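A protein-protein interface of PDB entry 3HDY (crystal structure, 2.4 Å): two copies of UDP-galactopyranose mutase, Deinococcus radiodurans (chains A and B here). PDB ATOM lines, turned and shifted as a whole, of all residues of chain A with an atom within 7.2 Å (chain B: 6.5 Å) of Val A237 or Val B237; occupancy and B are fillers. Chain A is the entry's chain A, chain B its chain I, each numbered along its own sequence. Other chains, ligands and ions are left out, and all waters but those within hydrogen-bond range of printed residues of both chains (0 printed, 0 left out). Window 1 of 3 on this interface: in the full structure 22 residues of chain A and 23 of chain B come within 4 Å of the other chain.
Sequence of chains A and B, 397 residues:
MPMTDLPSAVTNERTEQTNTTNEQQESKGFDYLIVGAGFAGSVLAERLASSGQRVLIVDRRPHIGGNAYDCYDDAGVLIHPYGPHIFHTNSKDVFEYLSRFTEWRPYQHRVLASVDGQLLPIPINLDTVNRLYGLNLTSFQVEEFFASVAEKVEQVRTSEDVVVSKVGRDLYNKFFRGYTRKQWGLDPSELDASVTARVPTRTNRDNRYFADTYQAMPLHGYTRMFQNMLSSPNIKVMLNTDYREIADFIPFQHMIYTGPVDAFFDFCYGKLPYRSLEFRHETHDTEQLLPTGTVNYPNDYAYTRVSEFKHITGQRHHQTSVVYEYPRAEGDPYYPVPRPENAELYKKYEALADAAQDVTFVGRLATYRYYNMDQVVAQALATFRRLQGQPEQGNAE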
ATOM      1  N   ALA A  37      11.078  26.153   2.633  1.00  0.00           N
ATOM      2  CA  ALA A  37      12.368  25.896   2.003  1.00  0.00           C
ATOM      3  C   ALA A  37      12.894  27.136   1.290  1.00  0.00           C
ATOM      4  O   ALA A  37      13.706  27.037   0.372  1.00  0.00           O
ATOM      5  CB  ALA A  37      12.264  24.729   1.036  1.00  0.00           C
ATOM      6  N   VAL A  55      18.111  17.988  11.056  1.00  0.00           N
ATOM      7  CA  VAL A  55      17.076  18.886  10.579  1.00  0.00           C
ATOM      8  C   VAL A  55      16.131  18.212   9.597  1.00  0.00           C
ATOM      9  O   VAL A  55      16.559  17.491   8.694  1.00  0.00           O
ATOM     10  CB  VAL A  55      17.696  20.131   9.908  1.00  0.00           C
ATOM     11  CG1 VAL A  55      16.616  21.013   9.313  1.00  0.00           C
ATOM     12  CG2 VAL A  55      18.533  20.910  10.907  1.00  0.00           C
ATOM     13  N   LEU A  56      14.839  18.444   9.793  1.00  0.00           N
ATOM     14  CA  LEU A  56      13.849  18.090   8.795  1.00  0.00           C
ATOM     15  C   LEU A  56      13.231  19.370   8.265  1.00  0.00           C
ATOM     16  O   LEU A  56      12.467  20.039   8.961  1.00  0.00           O
ATOM     17  CB  LEU A  56      12.763  17.194   9.380  1.00  0.00           C
ATOM     18  CG  LEU A  56      11.622  16.890   8.409  1.00  0.00           C
ATOM     19  CD1 LEU A  56      12.140  16.133   7.200  1.00  0.00           C
ATOM     20  CD2 LEU A  56      10.528  16.104   9.103  1.00  0.00           C
ATOM     21  N   ILE A  57      13.580  19.718   7.034  1.00  0.00           N
ATOM     22  CA  ILE A  57      13.016  20.894   6.394  1.00  0.00           C
ATOM     23  C   ILE A  57      11.880  20.454   5.474  1.00  0.00           C
ATOM     24  O   ILE A  57      12.045  19.553   4.653  1.00  0.00           O
ATOM     25  CB  ILE A  57      14.092  21.692   5.631  1.00  0.00           C
ATOM     26  CG1 ILE A  57      13.550  23.057   5.210  1.00  0.00           C
ATOM     27  CG2 ILE A  57      14.617  20.900   4.439  1.00  0.00           C
ATOM     28  CD1 ILE A  57      14.617  24.001   4.688  1.00  0.00           C
ATOM     29  N   VAL A  58      10.721  21.083   5.634  1.00  0.00           N
ATOM     30  CA  VAL A  58       9.513  20.664   4.938  1.00  0.00           C
ATOM     31  C   VAL A  58       8.893  21.847   4.201  1.00  0.00           C
ATOM     32  O   VAL A  58       9.044  22.994   4.624  1.00  0.00           O
ATOM     33  CB  VAL A  58       8.482  20.094   5.935  1.00  0.00           C
ATOM     34  CG1 VAL A  58       7.948  21.201   6.831  1.00  0.00           C
ATOM     35  CG2 VAL A  58       7.344  19.407   5.202  1.00  0.00           C
ATOM     36  N   ASP A  59       8.205  21.571   3.098  1.00  0.00           N
ATOM     37  CA  ASP A  59       7.530  22.624   2.342  1.00  0.00           C
ATOM     38  C   ASP A  59       6.336  22.067   1.573  1.00  0.00           C
ATOM     39  O   ASP A  59       6.406  20.978   1.003  1.00  0.00           O
ATOM     40  CB  ASP A  59       8.506  23.324   1.390  1.00  0.00           C
ATOM     41  CG  ASP A  59       7.958  24.636   0.842  1.00  0.00           C
ATOM     42  OD1 ASP A  59       6.866  24.621   0.234  1.00  0.00           O
ATOM     43  OD2 ASP A  59       8.627  25.679   1.012  1.00  0.00           O
ATOM     44  N   PRO A  62       6.298  21.564  -4.170  1.00  0.00           N
ATOM     45  CA  PRO A  62       7.071  20.397  -4.612  1.00  0.00           C
ATOM     46  C   PRO A  62       8.527  20.740  -4.936  1.00  0.00           C
ATOM     47  O   PRO A  62       9.189  19.986  -5.646  1.00  0.00           O
ATOM     48  CB  PRO A  62       6.354  19.967  -5.904  1.00  0.00           C
ATOM     49  CG  PRO A  62       5.224  20.964  -6.113  1.00  0.00           C
ATOM     50  CD  PRO A  62       5.542  22.158  -5.281  1.00  0.00           C
ATOM     51  N   HIS A  63       9.012  21.868  -4.431  1.00  0.00           N
ATOM     52  CA  HIS A  63      10.367  22.311  -4.723  1.00  0.00           C
ATOM     53  C   HIS A  63      10.897  23.193  -3.603  1.00  0.00           C
ATOM     54  O   HIS A  63      10.132  23.747  -2.812  1.00  0.00           O
ATOM     55  CB  HIS A  63      10.382  23.107  -6.021  1.00  0.00           C
ATOM     56  CG  HIS A  63       9.541  24.342  -5.967  1.00  0.00           C
ATOM     57  ND1 HIS A  63       9.948  25.490  -5.321  1.00  0.00           N
ATOM     58  CD2 HIS A  63       8.308  24.604  -6.460  1.00  0.00           C
ATOM     59  CE1 HIS A  63       9.005  26.409  -5.426  1.00  0.00           C
ATOM     60  NE2 HIS A  63       7.999  25.897  -6.111  1.00  0.00           N
ATOM     61  N   ILE A  64      12.215  23.333  -3.558  1.00  0.00           N
ATOM     62  CA  ILE A  64      12.875  24.187  -2.581  1.00  0.00           C
ATOM     63  C   ILE A  64      13.012  25.623  -3.102  1.00  0.00           C
ATOM     64  O   ILE A  64      12.729  25.895  -4.272  1.00  0.00           O
ATOM     65  CB  ILE A  64      14.265  23.626  -2.238  1.00  0.00           C
ATOM     66  CG1 ILE A  64      15.159  23.629  -3.478  1.00  0.00           C
ATOM     67  CG2 ILE A  64      14.138  22.215  -1.712  1.00  0.00           C
ATOM     68  CD1 ILE A  64      16.487  22.939  -3.279  1.00  0.00           C
ATOM     69  N   LEU A 230      21.201  22.799   1.089  1.00  0.00           N
ATOM     70  CA  LEU A 230      20.500  21.762   1.841  1.00  0.00           C
ATOM     71  C   LEU A 230      21.117  20.386   1.596  1.00  0.00           C
ATOM     72  O   LEU A 230      20.471  19.358   1.800  1.00  0.00           O
ATOM     73  CB  LEU A 230      19.019  21.737   1.449  1.00  0.00           C
ATOM     74  CG  LEU A 230      18.249  23.055   1.516  1.00  0.00           C
ATOM     75  CD1 LEU A 230      16.840  22.869   0.987  1.00  0.00           C
ATOM     76  CD2 LEU A 230      18.216  23.580   2.939  1.00  0.00           C
ATOM     77  N   SER A 231      22.372  20.371   1.162  1.00  0.00           N
ATOM     78  CA  SER A 231      22.992  19.138   0.691  1.00  0.00           C
ATOM     79  C   SER A 231      23.553  18.270   1.814  1.00  0.00           C
ATOM     80  O   SER A 231      23.833  17.089   1.603  1.00  0.00           O
ATOM     81  CB  SER A 231      24.091  19.452  -0.323  1.00  0.00           C
ATOM     82  OG  SER A 231      25.206  20.044   0.314  1.00  0.00           O
ATOM     83  N   SER A 232      23.717  18.858   2.997  1.00  0.00           N
ATOM     84  CA  SER A 232      24.283  18.144   4.145  1.00  0.00           C
ATOM     85  C   SER A 232      23.486  16.903   4.540  1.00  0.00           C
ATOM     86  O   SER A 232      22.257  16.902   4.488  1.00  0.00           O
ATOM     87  CB  SER A 232      24.398  19.070   5.355  1.00  0.00           C
ATOM     88  OG  SER A 232      24.612  18.322   6.540  1.00  0.00           O
ATOM     89  N   ILE A 235      20.534  17.055   6.965  1.00  0.00           N
ATOM     90  CA  ILE A 235      19.268  17.653   6.554  1.00  0.00           C
ATOM     91  C   ILE A 235      18.390  16.688   5.760  1.00  0.00           C
ATOM     92  O   ILE A 235      18.833  16.106   4.771  1.00  0.00           O
ATOM     93  CB  ILE A 235      19.511  18.921   5.717  1.00  0.00           C
ATOM     94  CG1 ILE A 235      20.395  19.899   6.493  1.00  0.00           C
ATOM     95  CG2 ILE A 235      18.193  19.564   5.323  1.00  0.00           C
ATOM     96  CD1 ILE A 235      20.836  21.099   5.696  1.00  0.00           C
ATOM     97  N   LYS A 236      17.147  16.520   6.201  1.00  0.00           N
ATOM     98  CA  LYS A 236      16.155  15.754   5.448  1.00  0.00           C
ATOM     99  C   LYS A 236      15.144  16.710   4.820  1.00  0.00           C
ATOM    100  O   LYS A 236      14.532  17.526   5.514  1.00  0.00           O
ATOM    101  CB  LYS A 236      15.435  14.740   6.347  1.00  0.00           C
ATOM    102  CG  LYS A 236      16.358  13.801   7.096  1.00  0.00           C
ATOM    103  CD  LYS A 236      17.323  13.118   6.145  1.00  0.00           C
ATOM    104  CE  LYS A 236      18.682  12.903   6.793  1.00  0.00           C
ATOM    105  NZ  LYS A 236      19.719  12.486   5.803  1.00  0.00           N
ATOM    106  N   VAL A 237      14.971  16.609   3.506  1.00  0.00           N
ATOM    107  CA  VAL A 237      14.092  17.521   2.779  1.00  0.00           C
ATOM    108  C   VAL A 237      12.769  16.864   2.442  1.00  0.00           C
ATOM    109  O   VAL A 237      12.739  15.821   1.793  1.00  0.00           O
ATOM    110  CB  VAL A 237      14.737  17.989   1.470  1.00  0.00           C
ATOM    111  CG1 VAL A 237      13.730  18.758   0.628  1.00  0.00           C
ATOM    112  CG2 VAL A 237      15.967  18.828   1.765  1.00  0.00           C
ATOM    113  N   MET A 238      11.676  17.483   2.879  1.00  0.00           N
ATOM    114  CA  MET A 238      10.343  16.945   2.635  1.00  0.00           C
ATOM    115  C   MET A 238       9.503  17.902   1.790  1.00  0.00           C
ATOM    116  O   MET A 238       9.272  19.049   2.173  1.00  0.00           O
ATOM    117  CB  MET A 238       9.636  16.630   3.956  1.00  0.00           C
ATOM    118  CG  MET A 238       8.478  15.659   3.808  1.00  0.00           C
ATOM    119  SD  MET A 238       7.864  15.056   5.392  1.00  0.00           S
ATOM    120  CE  MET A 238       6.726  13.789   4.842  1.00  0.00           C
ATOM    121  N   LEU A 239       9.048  17.420   0.637  1.00  0.00           N
ATOM    122  CA  LEU A 239       8.332  18.270  -0.314  1.00  0.00           C
ATOM    123  C   LEU A 239       6.867  17.863  -0.489  1.00  0.00           C
ATOM    124  O   LEU A 239       6.494  16.718  -0.230  1.00  0.00           O
ATOM    125  CB  LEU A 239       9.058  18.282  -1.662  1.00  0.00           C
ATOM    126  CG  LEU A 239      10.509  18.770  -1.613  1.00  0.00           C
ATOM    127  CD1 LEU A 239      11.113  18.830  -3.007  1.00  0.00           C
ATOM    128  CD2 LEU A 239      10.592  20.130  -0.938  1.00  0.00           C
ATOM    129  N   ASN A 240       6.043  18.815  -0.922  1.00  0.00           N
ATOM    130  CA  ASN A 240       4.616  18.584  -1.126  1.00  0.00           C
ATOM    131  C   ASN A 240       3.900  18.281   0.182  1.00  0.00           C
ATOM    132  O   ASN A 240       2.936  17.513   0.214  1.00  0.00           O
ATOM    133  CB  ASN A 240       4.389  17.443  -2.120  1.00  0.00           C
ATOM    134  CG  ASN A 240       3.008  17.471  -2.730  1.00  0.00           C
ATOM    135  OD1 ASN A 240       2.519  18.526  -3.140  1.00  0.00           O
ATOM    136  ND2 ASN A 240       2.368  16.309  -2.799  1.00  0.00           N
ATOM    137  N   THR A 241       4.371  18.897   1.260  1.00  0.00           N
ATOM    138  CA  THR A 241       3.911  18.545   2.597  1.00  0.00           C
ATOM    139  C   THR A 241       3.699  19.762   3.494  1.00  0.00           C
ATOM    140  O   THR A 241       4.656  20.440   3.863  1.00  0.00           O
ATOM    141  CB  THR A 241       4.921  17.608   3.287  1.00  0.00           C
ATOM    142  OG1 THR A 241       5.163  16.468   2.453  1.00  0.00           O
ATOM    143  CG2 THR A 241       4.398  17.146   4.635  1.00  0.00           C
ATOM    144  N   ALA B  37      12.638   6.539  -5.299  1.00  0.00           N
ATOM    145  CA  ALA B  37      11.779   7.384  -6.124  1.00  0.00           C
ATOM    146  C   ALA B  37      12.030   7.233  -7.626  1.00  0.00           C
ATOM    147  O   ALA B  37      11.798   8.165  -8.395  1.00  0.00           O
ATOM    148  CB  ALA B  37      11.915   8.845  -5.706  1.00  0.00           C
ATOM    149  N   VAL B  55       0.594   8.042   0.874  1.00  0.00           N
ATOM    150  CA  VAL B  55       1.915   7.506   0.592  1.00  0.00           C
ATOM    151  C   VAL B  55       3.031   8.470   0.961  1.00  0.00           C
ATOM    152  O   VAL B  55       2.979   9.658   0.637  1.00  0.00           O
ATOM    153  CB  VAL B  55       2.061   7.139  -0.894  1.00  0.00           C
ATOM    154  CG1 VAL B  55       3.460   6.613  -1.177  1.00  0.00           C
ATOM    155  CG2 VAL B  55       1.012   6.116  -1.289  1.00  0.00           C
ATOM    156  N   LEU B  56       4.036   7.940   1.646  1.00  0.00           N
ATOM    157  CA  LEU B  56       5.271   8.663   1.893  1.00  0.00           C
ATOM    158  C   LEU B  56       6.390   8.002   1.099  1.00  0.00           C
ATOM    159  O   LEU B  56       6.805   6.889   1.416  1.00  0.00           O
ATOM    160  CB  LEU B  56       5.612   8.650   3.382  1.00  0.00           C
ATOM    161  CG  LEU B  56       7.001   9.184   3.746  1.00  0.00           C
ATOM    162  CD1 LEU B  56       7.266  10.526   3.071  1.00  0.00           C
ATOM    163  CD2 LEU B  56       7.164   9.291   5.255  1.00  0.00           C
ATOM    164  N   ILE B  57       6.871   8.678   0.062  1.00  0.00           N
ATOM    165  CA  ILE B  57       7.970   8.143  -0.741  1.00  0.00           C
ATOM    166  C   ILE B  57       9.292   8.834  -0.412  1.00  0.00           C
ATOM    167  O   ILE B  57       9.380  10.064  -0.395  1.00  0.00           O
ATOM    168  CB  ILE B  57       7.689   8.239  -2.256  1.00  0.00           C
ATOM    169  CG1 ILE B  57       8.862   7.662  -3.049  1.00  0.00           C
ATOM    170  CG2 ILE B  57       7.421   9.682  -2.662  1.00  0.00           C
ATOM    171  CD1 ILE B  57       8.533   7.352  -4.492  1.00  0.00           C
ATOM    172  N   VAL B  58      10.320   8.035  -0.154  1.00  0.00           N
ATOM    173  CA  VAL B  58      11.601   8.576   0.274  1.00  0.00           C
ATOM    174  C   VAL B  58      12.752   8.118  -0.618  1.00  0.00           C
ATOM    175  O   VAL B  58      12.669   7.084  -1.274  1.00  0.00           O
ATOM    176  CB  VAL B  58      11.891   8.197   1.734  1.00  0.00           C
ATOM    177  CG1 VAL B  58      12.368   6.755   1.825  1.00  0.00           C
ATOM    178  CG2 VAL B  58      12.916   9.143   2.326  1.00  0.00           C
ATOM    179  N   ILE B  64      14.380  13.011  -7.384  1.00  0.00           N
ATOM    180  CA  ILE B  64      13.494  11.895  -7.681  1.00  0.00           C
ATOM    181  C   ILE B  64      13.916  11.285  -9.005  1.00  0.00           C
ATOM    182  O   ILE B  64      14.922  11.691  -9.585  1.00  0.00           O
ATOM    183  CB  ILE B  64      12.036  12.362  -7.797  1.00  0.00           C
ATOM    184  CG1 ILE B  64      11.920  13.468  -8.849  1.00  0.00           C
ATOM    185  CG2 ILE B  64      11.536  12.865  -6.454  1.00  0.00           C
ATOM    186  CD1 ILE B  64      10.501  13.882  -9.157  1.00  0.00           C
ATOM    187  N   LEU B 230       4.115  12.166  -9.391  1.00  0.00           N
ATOM    188  CA  LEU B 230       4.115  12.265  -7.933  1.00  0.00           C
ATOM    189  C   LEU B 230       3.360  13.483  -7.407  1.00  0.00           C
ATOM    190  O   LEU B 230       3.596  13.931  -6.283  1.00  0.00           O
ATOM    191  CB  LEU B 230       5.550  12.296  -7.403  1.00  0.00           C
ATOM    192  CG  LEU B 230       6.404  11.043  -7.609  1.00  0.00           C
ATOM    193  CD1 LEU B 230       7.799  11.261  -7.049  1.00  0.00           C
ATOM    194  CD2 LEU B 230       5.748   9.836  -6.966  1.00  0.00           C
ATOM    195  N   ILE B 235       0.638  12.156  -1.797  1.00  0.00           N
ATOM    196  CA  ILE B 235       2.038  11.749  -1.872  1.00  0.00           C
ATOM    197  C   ILE B 235       2.984  12.750  -1.218  1.00  0.00           C
ATOM    198  O   ILE B 235       3.124  13.881  -1.681  1.00  0.00           O
ATOM    199  CB  ILE B 235       2.485  11.538  -3.322  1.00  0.00           C
ATOM    200  CG1 ILE B 235       1.669  10.429  -3.979  1.00  0.00           C
ATOM    201  CG2 ILE B 235       3.967  11.205  -3.370  1.00  0.00           C
ATOM    202  CD1 ILE B 235       2.071  10.160  -5.407  1.00  0.00           C
ATOM    203  N   LYS B 236       3.635  12.326  -0.141  1.00  0.00           N
ATOM    204  CA  LYS B 236       4.658  13.145   0.488  1.00  0.00           C
ATOM    205  C   LYS B 236       6.034  12.661   0.045  1.00  0.00           C
ATOM    206  O   LYS B 236       6.333  11.467   0.102  1.00  0.00           O
ATOM    207  CB  LYS B 236       4.530  13.110   2.011  1.00  0.00           C
ATOM    208  CG  LYS B 236       3.159  13.524   2.521  1.00  0.00           C
ATOM    209  CD  LYS B 236       2.663  14.764   1.800  1.00  0.00           C
ATOM    210  CE  LYS B 236       1.189  15.015   2.085  1.00  0.00           C
ATOM    211  NZ  LYS B 236       0.643  16.174   1.316  1.00  0.00           N
ATOM    212  N   VAL B 237       6.862  13.591  -0.414  1.00  0.00           N
ATOM    213  CA  VAL B 237       8.165  13.245  -0.959  1.00  0.00           C
ATOM    214  C   VAL B 237       9.262  13.650   0.011  1.00  0.00           C
ATOM    215  O   VAL B 237       9.277  14.775   0.509  1.00  0.00           O
ATOM    216  CB  VAL B 237       8.418  13.937  -2.317  1.00  0.00           C
ATOM    217  CG1 VAL B 237       9.744  13.477  -2.904  1.00  0.00           C
ATOM    218  CG2 VAL B 237       7.271  13.666  -3.284  1.00  0.00           C
ATOM    219  N   MET B 238      10.180  12.725   0.273  1.00  0.00           N
ATOM    220  CA  MET B 238      11.280  12.979   1.188  1.00  0.00           C
ATOM    221  C   MET B 238      12.605  12.607   0.538  1.00  0.00           C
ATOM    222  O   MET B 238      12.842  11.449   0.205  1.00  0.00           O
ATOM    223  CB  MET B 238      11.073  12.202   2.485  1.00  0.00           C
ATOM    224  CG  MET B 238      11.969  12.645   3.618  1.00  0.00           C
ATOM    225  SD  MET B 238      11.324  12.117   5.212  1.00  0.00           S
ATOM    226  CE  MET B 238      12.612  12.719   6.292  1.00  0.00           C
ATOM    227  N   LEU B 239      13.467  13.604   0.358  1.00  0.00           N
ATOM    228  CA  LEU B 239      14.708  13.430  -0.386  1.00  0.00           C
ATOM    229  C   LEU B 239      15.923  13.510   0.528  1.00  0.00           C
ATOM    230  O   LEU B 239      15.827  14.007   1.649  1.00  0.00           O
ATOM    231  CB  LEU B 239      14.812  14.492  -1.482  1.00  0.00           C
ATOM    232  CG  LEU B 239      13.689  14.511  -2.521  1.00  0.00           C
ATOM    233  CD1 LEU B 239      13.715  15.801  -3.340  1.00  0.00           C
ATOM    234  CD2 LEU B 239      13.772  13.293  -3.423  1.00  0.00           C
ATOM    235  N   ASN B 240      17.061  13.019   0.040  1.00  0.00           N
ATOM    236  CA  ASN B 240      18.316  13.095   0.781  1.00  0.00           C
ATOM    237  C   ASN B 240      18.212  12.284   2.068  1.00  0.00           C
ATOM    238  O   ASN B 240      18.859  12.593   3.069  1.00  0.00           O
ATOM    239  CB  ASN B 240      18.652  14.560   1.089  1.00  0.00           C
ATOM    240  CG  ASN B 240      20.062  14.745   1.616  1.00  0.00           C
ATOM    241  OD1 ASN B 240      20.959  13.953   1.323  1.00  0.00           O
ATOM    242  ND2 ASN B 240      20.265  15.801   2.394  1.00  0.00           N
ATOM    243  N   THR B 241      17.396  11.235   2.024  1.00  0.00           N
ATOM    244  CA  THR B 241      17.009  10.502   3.224  1.00  0.00           C
ATOM    245  C   THR B 241      17.082   8.991   3.038  1.00  0.00           C
ATOM    246  O   THR B 241      16.423   8.432   2.164  1.00  0.00           O
ATOM    247  CB  THR B 241      15.563  10.860   3.645  1.00  0.00           C
ATOM    248  OG1 THR B 241      15.470  12.261   3.938  1.00  0.00           O
ATOM    249  CG2 THR B 241      15.141  10.056   4.865  1.00  0.00           C
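O of Val A237 is in hydrogen-bond range of N of Leu B239. O of Asn A240 sits at hydrogen-bond distance from NZ of Lys B236, 2.9 Å away. The side-chain amino group (NZ) of Lys A236 lies within hydrogen-bond range of the backbone carbonyl oxygen (O) of Asn B240. The backbone carbonyl oxygen (O) of Val B237 is in hydrogen-bond range of the backbone NH (N) of Leu A239, at 2.7 Å. The side-chain amide nitrogen (ND2) of Asn B240 sits at hydrogen-bond distance from the backbone carbonyl oxygen (O) of Ser A232 (3.1 Å). O of Ile A235 sits at hydrogen-bond distance from ND2 of Asn B240, 2.8 Å away. The backbone carbonyl oxygen of Ile B235 lies within hydrogen-bond range of the side-chain amide nitrogen of Asn A240 (2.8 Å).
The side-chain hydroxyl (OG1) of Thr A241 is in hydrogen-bond range of the backbone carbonyl oxygen (O) of Leu A239, 3.0 Å away. O of Lys B236 is in hydrogen-bond range of N of Ile B57. The backbone carbonyl oxygen of Leu B239 is in hydrogen-bond range of the side-chain hydroxyl of Thr B241, at 2.9 Å. O of Val B55 lies within hydrogen-bond range of N of Lys B236 (2.9 Å). N of Thr A241 is in hydrogen-bond range of O of Asp A59 (2.9 Å). The backbone carbonyl oxygen of Ile A57 is in hydrogen-bond range of the backbone NH of Met A238 (2.8 Å).
Among the printed residues, pairs that only touch across the chains: Lys A236 with Thr B241 (3.0 Å), Thr A241 with Lys B236 (3.1 Å), Met A238 with Val B237 (3.2 Å), Val A237 with Met B238 (3.3 Å), Lys A236 with Met B238 (3.5 Å), Leu A56 with Met B238 (3.6 Å), Leu A230 with Asn B240 (3.6 Å), Met A238 with Lys B236 (3.6 Å), Met A238 with Leu B56 (3.8 Å), Val A237 with Val B237 (3.8 Å) and Ser A231 with Asn B240 (3.9 Å).
Val A237 touches just these residues of chain B: Val B237 (3.8 Å), Met B238 (3.3 Å) and Leu B239 (2.7 Å). Val B237 touches just these residues of chain A: Val A237 (3.8 Å), Met A238 (3.2 Å) and Leu A239 (2.7 Å). Of the printed residues of chain A, Asn B240 touches Leu A230, Ser A231, Ser A232, Ile A235 and Lys A236. Of the printed residues of chain B, Thr A241 touches Lys B236. Printed residues of chain A within 4 Å of Leu B239: Val A237. Of the printed residues of chain A, Ile B235 touches Asn A240 (2.8 Å). Printed residues of chain A within 4 Å of Lys B236: Met A238 (3.6 Å), Asn A240 (2.9 Å) and Thr A241 (3.1 Å). The nearest residue of chain A that does not touch Val B237 is Thr A241 (4.4 Å).
Of the 19 printed residues of chain A, 11 touch a printed residue of chain B. Hydrophobic or aromatic side chains of chain A that line the printed part of chain B: Leu A56 and Met A238. Of the 14 printed residues of chain B, 8 touch a printed residue of chain A. Among the printed residues, no Asp or Glu carboxylate lies within 4 Å of a Lys or Arg side-chain nitrogen of the other chain.
Ile A235 touches Asn B240, and with the chains exchanged Asn A240 touches Ile B235. Lys A236 touches Met B238, and with the chains exchanged Met A238 touches Lys B236. Lys A236 touches Asn B240, and with the chains exchanged Asn A240 touches Lys B236. Val A237 touches Met B238, and with the chains exchanged Met A238 touches Val B237. Positions printed for both chains: 37, 55, 56, 57, 58, 64, 230, 235, 236, 237, 238, 239, 240 and 241.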
